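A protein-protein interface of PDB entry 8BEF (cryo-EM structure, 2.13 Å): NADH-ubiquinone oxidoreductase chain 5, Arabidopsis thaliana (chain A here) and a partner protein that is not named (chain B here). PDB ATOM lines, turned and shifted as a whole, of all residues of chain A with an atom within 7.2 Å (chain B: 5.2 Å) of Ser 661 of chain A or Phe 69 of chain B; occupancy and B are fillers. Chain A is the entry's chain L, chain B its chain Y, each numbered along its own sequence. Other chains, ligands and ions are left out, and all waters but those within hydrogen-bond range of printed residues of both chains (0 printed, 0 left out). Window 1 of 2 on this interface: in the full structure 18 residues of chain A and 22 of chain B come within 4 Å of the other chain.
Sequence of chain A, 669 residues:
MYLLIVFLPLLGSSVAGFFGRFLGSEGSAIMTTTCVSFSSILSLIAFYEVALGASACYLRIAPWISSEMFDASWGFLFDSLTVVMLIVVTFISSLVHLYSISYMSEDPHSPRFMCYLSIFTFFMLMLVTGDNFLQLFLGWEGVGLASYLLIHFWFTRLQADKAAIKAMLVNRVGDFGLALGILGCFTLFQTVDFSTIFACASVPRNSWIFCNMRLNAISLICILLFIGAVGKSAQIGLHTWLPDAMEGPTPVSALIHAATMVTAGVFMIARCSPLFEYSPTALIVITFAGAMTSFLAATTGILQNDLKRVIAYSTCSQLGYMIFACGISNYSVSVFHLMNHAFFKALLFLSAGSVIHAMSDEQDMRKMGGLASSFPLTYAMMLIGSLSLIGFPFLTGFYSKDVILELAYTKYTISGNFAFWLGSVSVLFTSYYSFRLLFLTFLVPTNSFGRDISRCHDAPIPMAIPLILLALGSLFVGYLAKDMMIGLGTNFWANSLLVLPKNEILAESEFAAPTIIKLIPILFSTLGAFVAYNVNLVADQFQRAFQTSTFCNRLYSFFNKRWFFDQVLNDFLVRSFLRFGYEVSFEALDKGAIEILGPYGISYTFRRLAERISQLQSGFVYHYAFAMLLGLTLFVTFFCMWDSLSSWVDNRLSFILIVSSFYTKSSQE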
ATOM      1  N   ARG A 612       0.476 -30.026 -17.070  1.00  0.00           N
ATOM      2  CA  ARG A 612       1.204 -28.965 -17.761  1.00  0.00           C
ATOM      3  C   ARG A 612       2.019 -28.120 -16.788  1.00  0.00           C
ATOM      4  O   ARG A 612       3.166 -27.760 -17.077  1.00  0.00           O
ATOM      5  CB  ARG A 612       0.219 -28.092 -18.542  1.00  0.00           C
ATOM      6  CG  ARG A 612      -0.180 -28.665 -19.894  1.00  0.00           C
ATOM      7  CD  ARG A 612      -1.123 -27.739 -20.645  1.00  0.00           C
ATOM      8  NE  ARG A 612      -0.450 -26.682 -21.393  1.00  0.00           N
ATOM      9  CZ  ARG A 612      -1.039 -25.559 -21.782  1.00  0.00           C
ATOM     10  NH1 ARG A 612      -2.300 -25.299 -21.478  1.00  0.00           N
ATOM     11  NH2 ARG A 612      -0.349 -24.677 -22.498  1.00  0.00           N
ATOM     12  N   LEU A 653      -8.123  -6.786 -23.881  1.00  0.00           N
ATOM     13  CA  LEU A 653      -7.253  -7.522 -24.809  1.00  0.00           C
ATOM     14  C   LEU A 653      -6.109  -8.152 -23.972  1.00  0.00           C
ATOM     15  O   LEU A 653      -5.891  -9.321 -24.165  1.00  0.00           O
ATOM     16  CB  LEU A 653      -6.697  -6.607 -25.902  1.00  0.00           C
ATOM     17  CG  LEU A 653      -7.714  -6.045 -26.898  1.00  0.00           C
ATOM     18  CD1 LEU A 653      -7.053  -5.043 -27.832  1.00  0.00           C
ATOM     19  CD2 LEU A 653      -8.371  -7.168 -27.687  1.00  0.00           C
ATOM     20  N   PHE A 655      -6.014  -9.365 -20.887  1.00  0.00           N
ATOM     21  CA  PHE A 655      -6.367 -10.628 -20.207  1.00  0.00           C
ATOM     22  C   PHE A 655      -6.813 -11.692 -21.231  1.00  0.00           C
ATOM     23  O   PHE A 655      -6.437 -12.859 -21.048  1.00  0.00           O
ATOM     24  CB  PHE A 655      -7.327 -10.354 -19.047  1.00  0.00           C
ATOM     25  CG  PHE A 655      -6.718  -9.728 -17.823  1.00  0.00           C
ATOM     26  CD1 PHE A 655      -5.912 -10.467 -16.974  1.00  0.00           C
ATOM     27  CD2 PHE A 655      -6.952  -8.398 -17.519  1.00  0.00           C
ATOM     28  CE1 PHE A 655      -5.351  -9.885 -15.849  1.00  0.00           C
ATOM     29  CE2 PHE A 655      -6.389  -7.819 -16.395  1.00  0.00           C
ATOM     30  CZ  PHE A 655      -5.588  -8.562 -15.564  1.00  0.00           C
ATOM     31  N   ILE A 656      -7.506 -11.310 -22.284  1.00  0.00           N
ATOM     32  CA  ILE A 656      -7.906 -12.253 -23.362  1.00  0.00           C
ATOM     33  C   ILE A 656      -6.699 -12.980 -23.958  1.00  0.00           C
ATOM     34  O   ILE A 656      -6.752 -14.211 -24.104  1.00  0.00           O
ATOM     35  CB  ILE A 656      -8.624 -11.459 -24.450  1.00  0.00           C
ATOM     36  CG1 ILE A 656      -9.834 -10.697 -23.900  1.00  0.00           C
ATOM     37  CG2 ILE A 656      -9.040 -12.323 -25.632  1.00  0.00           C
ATOM     38  CD1 ILE A 656     -10.886 -11.562 -23.255  1.00  0.00           C
ATOM     39  N   LEU A 657      -5.660 -12.222 -24.312  1.00  0.00           N
ATOM     40  CA  LEU A 657      -4.501 -12.853 -24.990  1.00  0.00           C
ATOM     41  C   LEU A 657      -3.854 -13.820 -23.976  1.00  0.00           C
ATOM     42  O   LEU A 657      -3.620 -14.967 -24.339  1.00  0.00           O
ATOM     43  CB  LEU A 657      -3.664 -11.686 -25.538  1.00  0.00           C
ATOM     44  CG  LEU A 657      -4.184 -11.093 -26.841  1.00  0.00           C
ATOM     45  CD1 LEU A 657      -3.328  -9.937 -27.296  1.00  0.00           C
ATOM     46  CD2 LEU A 657      -4.291 -12.150 -27.930  1.00  0.00           C
ATOM     47  N   ILE A 658      -3.843 -13.494 -22.685  1.00  0.00           N
ATOM     48  CA  ILE A 658      -3.241 -14.366 -21.678  1.00  0.00           C
ATOM     49  C   ILE A 658      -3.973 -15.701 -21.629  1.00  0.00           C
ATOM     50  O   ILE A 658      -3.356 -16.772 -21.687  1.00  0.00           O
ATOM     51  CB  ILE A 658      -3.234 -13.679 -20.301  1.00  0.00           C
ATOM     52  CG1 ILE A 658      -2.171 -12.580 -20.259  1.00  0.00           C
ATOM     53  CG2 ILE A 658      -2.988 -14.696 -19.198  1.00  0.00           C
ATOM     54  CD1 ILE A 658      -0.832 -13.005 -20.812  1.00  0.00           C
ATOM     55  N   VAL A 659      -5.302 -15.655 -21.531  1.00  0.00           N
ATOM     56  CA  VAL A 659      -6.090 -16.883 -21.510  1.00  0.00           C
ATOM     57  C   VAL A 659      -5.960 -17.622 -22.836  1.00  0.00           C
ATOM     58  O   VAL A 659      -5.828 -18.851 -22.868  1.00  0.00           O
ATOM     59  CB  VAL A 659      -7.559 -16.565 -21.171  1.00  0.00           C
ATOM     60  CG1 VAL A 659      -8.494 -17.592 -21.788  1.00  0.00           C
ATOM     61  CG2 VAL A 659      -7.751 -16.502 -19.665  1.00  0.00           C
ATOM     62  N   SER A 660      -5.984 -16.883 -23.948  1.00  0.00           N
ATOM     63  CA  SER A 660      -5.886 -17.514 -25.260  1.00  0.00           C
ATOM     64  C   SER A 660      -4.590 -18.295 -25.423  1.00  0.00           C
ATOM     65  O   SER A 660      -4.543 -19.260 -26.191  1.00  0.00           O
ATOM     66  CB  SER A 660      -6.007 -16.462 -26.361  1.00  0.00           C
ATOM     67  OG  SER A 660      -5.595 -16.986 -27.608  1.00  0.00           O
ATOM     68  N   SER A 661      -3.531 -17.899 -24.710  1.00  0.00           N
ATOM     69  CA  SER A 661      -2.256 -18.602 -24.821  1.00  0.00           C
ATOM     70  C   SER A 661      -2.373 -20.059 -24.396  1.00  0.00           C
ATOM     71  O   SER A 661      -1.582 -20.898 -24.837  1.00  0.00           O
ATOM     72  CB  SER A 661      -1.189 -17.898 -23.984  1.00  0.00           C
ATOM     73  OG  SER A 661      -1.127 -16.517 -24.289  1.00  0.00           O
ATOM     74  N   PHE A 662      -3.350 -20.378 -23.544  1.00  0.00           N
ATOM     75  CA  PHE A 662      -3.507 -21.752 -23.080  1.00  0.00           C
ATOM     76  C   PHE A 662      -3.829 -22.695 -24.230  1.00  0.00           C
ATOM     77  O   PHE A 662      -3.476 -23.878 -24.182  1.00  0.00           O
ATOM     78  CB  PHE A 662      -4.600 -21.823 -22.015  1.00  0.00           C
ATOM     79  CG  PHE A 662      -4.326 -20.984 -20.793  1.00  0.00           C
ATOM     80  CD1 PHE A 662      -3.046 -20.542 -20.505  1.00  0.00           C
ATOM     81  CD2 PHE A 662      -5.357 -20.637 -19.936  1.00  0.00           C
ATOM     82  CE1 PHE A 662      -2.800 -19.769 -19.385  1.00  0.00           C
ATOM     83  CE2 PHE A 662      -5.117 -19.865 -18.816  1.00  0.00           C
ATOM     84  CZ  PHE A 662      -3.836 -19.432 -18.540  1.00  0.00           C
ATOM     85  N   TYR A 663      -4.493 -22.194 -25.266  1.00  0.00           N
ATOM     86  CA  TYR A 663      -4.883 -23.005 -26.418  1.00  0.00           C
ATOM     87  C   TYR A 663      -3.881 -22.841 -27.558  1.00  0.00           C
ATOM     88  O   TYR A 663      -4.197 -22.355 -28.645  1.00  0.00           O
ATOM     89  CB  TYR A 663      -6.292 -22.635 -26.864  1.00  0.00           C
ATOM     90  CG  TYR A 663      -7.327 -22.776 -25.774  1.00  0.00           C
ATOM     91  CD1 TYR A 663      -7.566 -21.747 -24.878  1.00  0.00           C
ATOM     92  CD2 TYR A 663      -8.059 -23.945 -25.639  1.00  0.00           C
ATOM     93  CE1 TYR A 663      -8.508 -21.877 -23.885  1.00  0.00           C
ATOM     94  CE2 TYR A 663      -9.000 -24.082 -24.650  1.00  0.00           C
ATOM     95  CZ  TYR A 663      -9.222 -23.047 -23.774  1.00  0.00           C
ATOM     96  OH  TYR A 663     -10.164 -23.183 -22.784  1.00  0.00           O
ATOM     97  N   THR A 664      -2.649 -23.265 -27.296  1.00  0.00           N
ATOM     98  CA  THR A 664      -1.567 -23.191 -28.268  1.00  0.00           C
ATOM     99  C   THR A 664      -0.954 -24.573 -28.437  1.00  0.00           C
ATOM    100  O   THR A 664      -0.639 -25.240 -27.446  1.00  0.00           O
ATOM    101  CB  THR A 664      -0.503 -22.180 -27.830  1.00  0.00           C
ATOM    102  OG1 THR A 664      -0.970 -20.851 -28.096  1.00  0.00           O
ATOM    103  CG2 THR A 664       0.802 -22.408 -28.579  1.00  0.00           C
ATOM    104  N   LYS A 665      -0.795 -24.995 -29.690  1.00  0.00           N
ATOM    105  CA  LYS A 665      -0.228 -26.301 -30.024  1.00  0.00           C
ATOM    106  C   LYS A 665      -1.016 -27.435 -29.373  1.00  0.00           C
ATOM    107  O   LYS A 665      -2.240 -27.494 -29.481  1.00  0.00           O
ATOM    108  CB  LYS A 665       1.244 -26.375 -29.609  1.00  0.00           C
ATOM    109  CG  LYS A 665       2.169 -25.509 -30.445  1.00  0.00           C
ATOM    110  CD  LYS A 665       3.630 -25.779 -30.117  1.00  0.00           C
ATOM    111  CE  LYS A 665       4.274 -26.677 -31.161  1.00  0.00           C
ATOM    112  NZ  LYS A 665       3.829 -28.090 -31.026  1.00  0.00           N
ATOM    113  N   GLY B  26      -1.986  -7.094 -30.389  1.00  0.00           N
ATOM    114  CA  GLY B  26      -1.945  -8.542 -30.428  1.00  0.00           C
ATOM    115  C   GLY B  26      -0.697  -9.067 -31.107  1.00  0.00           C
ATOM    116  O   GLY B  26      -0.096 -10.035 -30.647  1.00  0.00           O
ATOM    117  N   PHE B  27      -0.281  -8.429 -32.205  1.00  0.00           N
ATOM    118  CA  PHE B  27       0.947  -8.852 -32.868  1.00  0.00           C
ATOM    119  C   PHE B  27       2.166  -8.635 -31.977  1.00  0.00           C
ATOM    120  O   PHE B  27       3.063  -9.482 -31.931  1.00  0.00           O
ATOM    121  CB  PHE B  27       1.125  -8.119 -34.197  1.00  0.00           C
ATOM    122  CG  PHE B  27       2.334  -8.568 -34.971  1.00  0.00           C
ATOM    123  CD1 PHE B  27       2.268  -9.670 -35.805  1.00  0.00           C
ATOM    124  CD2 PHE B  27       3.537  -7.894 -34.858  1.00  0.00           C
ATOM    125  CE1 PHE B  27       3.375 -10.088 -36.509  1.00  0.00           C
ATOM    126  CE2 PHE B  27       4.648  -8.310 -35.560  1.00  0.00           C
ATOM    127  CZ  PHE B  27       4.567  -9.408 -36.386  1.00  0.00           C
ATOM    128  N   ALA B  29       2.252  -8.568 -28.614  1.00  0.00           N
ATOM    129  CA  ALA B  29       2.196  -9.550 -27.540  1.00  0.00           C
ATOM    130  C   ALA B  29       2.530 -10.945 -28.051  1.00  0.00           C
ATOM    131  O   ALA B  29       3.219 -11.712 -27.371  1.00  0.00           O
ATOM    132  CB  ALA B  29       0.817  -9.532 -26.884  1.00  0.00           C
ATOM    133  N   GLY B  30       2.049 -11.292 -29.247  1.00  0.00           N
ATOM    134  CA  GLY B  30       2.357 -12.592 -29.816  1.00  0.00           C
ATOM    135  C   GLY B  30       3.819 -12.747 -30.183  1.00  0.00           C
ATOM    136  O   GLY B  30       4.387 -13.828 -30.042  1.00  0.00           O
ATOM    137  N   TYR B  33       5.526 -13.366 -26.891  1.00  0.00           N
ATOM    138  CA  TYR B  33       5.168 -14.697 -26.419  1.00  0.00           C
ATOM    139  C   TYR B  33       5.904 -15.779 -27.202  1.00  0.00           C
ATOM    140  O   TYR B  33       6.414 -16.743 -26.619  1.00  0.00           O
ATOM    141  CB  TYR B  33       3.651 -14.856 -26.529  1.00  0.00           C
ATOM    142  CG  TYR B  33       3.095 -16.201 -26.151  1.00  0.00           C
ATOM    143  CD1 TYR B  33       3.144 -16.651 -24.842  1.00  0.00           C
ATOM    144  CD2 TYR B  33       2.485 -17.006 -27.099  1.00  0.00           C
ATOM    145  CE1 TYR B  33       2.620 -17.876 -24.492  1.00  0.00           C
ATOM    146  CE2 TYR B  33       1.956 -18.230 -26.758  1.00  0.00           C
ATOM    147  CZ  TYR B  33       2.029 -18.663 -25.454  1.00  0.00           C
ATOM    148  OH  TYR B  33       1.505 -19.887 -25.109  1.00  0.00           O
ATOM    149  N   THR B  64       4.595 -16.614 -36.324  1.00  0.00           N
ATOM    150  CA  THR B  64       3.352 -17.369 -36.209  1.00  0.00           C
ATOM    151  C   THR B  64       2.530 -16.900 -35.016  1.00  0.00           C
ATOM    152  O   THR B  64       1.312 -16.691 -35.129  1.00  0.00           O
ATOM    153  CB  THR B  64       3.662 -18.863 -36.093  1.00  0.00           C
ATOM    154  OG1 THR B  64       3.892 -19.409 -37.398  1.00  0.00           O
ATOM    155  CG2 THR B  64       2.511 -19.605 -35.434  1.00  0.00           C
ATOM    156  N   HIS B  65       3.182 -16.705 -33.865  1.00  0.00           N
ATOM    157  CA  HIS B  65       2.439 -16.301 -32.679  1.00  0.00           C
ATOM    158  C   HIS B  65       1.972 -14.856 -32.783  1.00  0.00           C
ATOM    159  O   HIS B  65       0.868 -14.526 -32.336  1.00  0.00           O
ATOM    160  CB  HIS B  65       3.280 -16.537 -31.430  1.00  0.00           C
ATOM    161  CG  HIS B  65       3.156 -17.928 -30.896  1.00  0.00           C
ATOM    162  ND1 HIS B  65       4.027 -18.938 -31.244  1.00  0.00           N
ATOM    163  CD2 HIS B  65       2.239 -18.487 -30.073  1.00  0.00           C
ATOM    164  CE1 HIS B  65       3.661 -20.055 -30.643  1.00  0.00           C
ATOM    165  NE2 HIS B  65       2.580 -19.808 -29.926  1.00  0.00           N
ATOM    166  N   GLY B  66       2.779 -13.987 -33.395  1.00  0.00           N
ATOM    167  CA  GLY B  66       2.311 -12.643 -33.678  1.00  0.00           C
ATOM    168  C   GLY B  66       1.090 -12.640 -34.576  1.00  0.00           C
ATOM    169  O   GLY B  66       0.135 -11.904 -34.332  1.00  0.00           O
ATOM    170  N   LEU B  67       1.089 -13.494 -35.604  1.00  0.00           N
ATOM    171  CA  LEU B  67      -0.054 -13.575 -36.510  1.00  0.00           C
ATOM    172  C   LEU B  67      -1.312 -14.020 -35.774  1.00  0.00           C
ATOM    173  O   LEU B  67      -2.363 -13.374 -35.871  1.00  0.00           O
ATOM    174  CB  LEU B  67       0.260 -14.534 -37.661  1.00  0.00           C
ATOM    175  CG  LEU B  67       0.716 -13.951 -39.002  1.00  0.00           C
ATOM    176  CD1 LEU B  67      -0.466 -13.368 -39.768  1.00  0.00           C
ATOM    177  CD2 LEU B  67       1.802 -12.910 -38.805  1.00  0.00           C
ATOM    178  N   THR B  68      -1.224 -15.123 -35.024  1.00  0.00           N
ATOM    179  CA  THR B  68      -2.426 -15.622 -34.356  1.00  0.00           C
ATOM    180  C   THR B  68      -2.919 -14.650 -33.287  1.00  0.00           C
ATOM    181  O   THR B  68      -4.124 -14.379 -33.201  1.00  0.00           O
ATOM    182  CB  THR B  68      -2.192 -17.014 -33.762  1.00  0.00           C
ATOM    183  OG1 THR B  68      -3.294 -17.362 -32.914  1.00  0.00           O
ATOM    184  CG2 THR B  68      -0.926 -17.064 -32.952  1.00  0.00           C
ATOM    185  N   PHE B  69      -2.011 -14.091 -32.480  1.00  0.00           N
ATOM    186  CA  PHE B  69      -2.445 -13.163 -31.442  1.00  0.00           C
ATOM    187  C   PHE B  69      -2.985 -11.870 -32.033  1.00  0.00           C
ATOM    188  O   PHE B  69      -3.917 -11.286 -31.474  1.00  0.00           O
ATOM    189  CB  PHE B  69      -1.301 -12.868 -30.471  1.00  0.00           C
ATOM    190  CG  PHE B  69      -1.191 -13.857 -29.346  1.00  0.00           C
ATOM    191  CD1 PHE B  69      -1.763 -15.112 -29.452  1.00  0.00           C
ATOM    192  CD2 PHE B  69      -0.537 -13.521 -28.173  1.00  0.00           C
ATOM    193  CE1 PHE B  69      -1.668 -16.023 -28.420  1.00  0.00           C
ATOM    194  CE2 PHE B  69      -0.437 -14.426 -27.136  1.00  0.00           C
ATOM    195  CZ  PHE B  69      -1.007 -15.681 -27.262  1.00  0.00           C
ATOM    196  N   ALA B  70      -2.431 -11.410 -33.158  1.00  0.00           N
ATOM    197  CA  ALA B  70      -3.015 -10.269 -33.848  1.00  0.00           C
ATOM    198  C   ALA B  70      -4.419 -10.594 -34.330  1.00  0.00           C
ATOM    199  O   ALA B  70      -5.320  -9.754 -34.249  1.00  0.00           O
ATOM    200  CB  ALA B  70      -2.130  -9.851 -35.019  1.00  0.00           C
ATOM    201  N   ALA B  71      -4.622 -11.814 -34.833  1.00  0.00           N
ATOM    202  CA  ALA B  71      -5.949 -12.220 -35.279  1.00  0.00           C
ATOM    203  C   ALA B  71      -6.954 -12.167 -34.133  1.00  0.00           C
ATOM    204  O   ALA B  71      -8.044 -11.601 -34.279  1.00  0.00           O
ATOM    205  CB  ALA B  71      -5.894 -13.619 -35.888  1.00  0.00           C
ATOM    206  N   ILE B  72      -6.599 -12.741 -32.976  1.00  0.00           N
ATOM    207  CA  ILE B  72      -7.509 -12.671 -31.829  1.00  0.00           C
ATOM    208  C   ILE B  72      -7.745 -11.221 -31.415  1.00  0.00           C
ATOM    209  O   ILE B  72      -8.890 -10.789 -31.231  1.00  0.00           O
ATOM    210  CB  ILE B  72      -7.002 -13.509 -30.636  1.00  0.00           C
ATOM    211  CG1 ILE B  72      -6.985 -15.008 -30.942  1.00  0.00           C
ATOM    212  CG2 ILE B  72      -7.843 -13.235 -29.399  1.00  0.00           C
ATOM    213  CD1 ILE B  72      -5.610 -15.625 -30.985  1.00  0.00           C
ATOM    214  N   GLY B  73      -6.668 -10.440 -31.285  1.00  0.00           N
ATOM    215  CA  GLY B  73      -6.790  -9.081 -30.787  1.00  0.00           C
ATOM    216  C   GLY B  73      -7.515  -8.142 -31.724  1.00  0.00           C
ATOM    217  O   GLY B  73      -8.019  -7.107 -31.279  1.00  0.00           O
ATOM    218  N   GLY B  74      -7.576  -8.478 -33.007  1.00  0.00           N
ATOM    219  CA  GLY B  74      -8.327  -7.684 -33.950  1.00  0.00           C
ATOM    220  C   GLY B  74      -9.772  -8.118 -34.044  1.00  0.00           C
ATOM    221  O   GLY B  74     -10.673  -7.282 -33.946  1.00  0.00           O
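OH of Tyr 33 of chain B lies within hydrogen-bond range of O of Ser 661 of chain A (3.3 Å).
The backbone carbonyl oxygen (O) of Ile 658 of chain A sits close to the side-chain hydroxyl (OG) of Ser 661 of chain A (3.4 Å).
The side-chain hydroxyl of Thr 664 of chain A lies within hydrogen-bond range of the backbone carbonyl oxygen of Ser 661 of chain A, at 3.3 Å.
The backbone carbonyl oxygen of Leu 657 of chain A sits at hydrogen-bond distance from the side-chain hydroxyl of Ser 661 of chain A, 2.9 Å away.
Among the printed residues, merely in contact across the chains: Ser 661 of chain A with Phe 69 of chain B (3.1 Å), Thr 664 of chain A with His 65 of chain B (3.4 Å), Leu 653 of chain A with Gly 73 of chain B (3.6 Å), Ser 660 of chain A with Ile 72 of chain B (3.6 Å), Leu 657 of chain A with Phe 69 of chain B (3.7 Å), Leu 657 of chain A with Gly 26 of chain B (3.7 Å), Leu 657 of chain A with Ile 72 of chain B (3.99 Å) and Thr 664 of chain A with Tyr 33 of chain B (3.997 Å).
Of chain B, only Tyr 33 (3.3 Å) and Phe 69 (3.1 Å) come within 4 Å of Ser 661 of chain A.
Of chain A, only Leu 657 and Ser 661 come within 4 Å of Phe 69 of chain B.
Printed residues of chain B within 4 Å of Leu 657 of chain A: Gly 26 (3.7 Å), Phe 69 (3.7 Å) and Ile 72 (3.99 Å).
Of the printed residues of chain A, Ile 72 of chain B touches Leu 657 (3.99 Å) and Ser 660 (3.6 Å).
Of the printed residues of chain A, His 65 of chain B touches Thr 664.
Of the printed residues of chain A, Gly 73 of chain B touches Leu 653 (3.6 Å).
Of the printed residues of chain A, Tyr 33 of chain B touches Ser 661 (3.3 Å) and Thr 664 (3.997 Å).
Phe 655 of chain A touches none of the printed residues of chain B.
Leu 67 of chain B touches none of the printed residues of chain A.
The nearest residue of chain A that does not touch Phe 69 of chain B is Ser 660 of chain A (4.1 Å).
The nearest printed residue of chain B that does not touch Thr 664 of chain A is Phe 69 of chain B (4.9 Å).
Printed residues of chain B that touch a printed residue of chain A: Gly 26, Tyr 33, His 65, Phe 69, Ile 72 and Gly 73.
Among the printed residues, no Asp or Glu carboxylate lies within 4 Å of a Lys or Arg side-chain nitrogen of the other chain.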
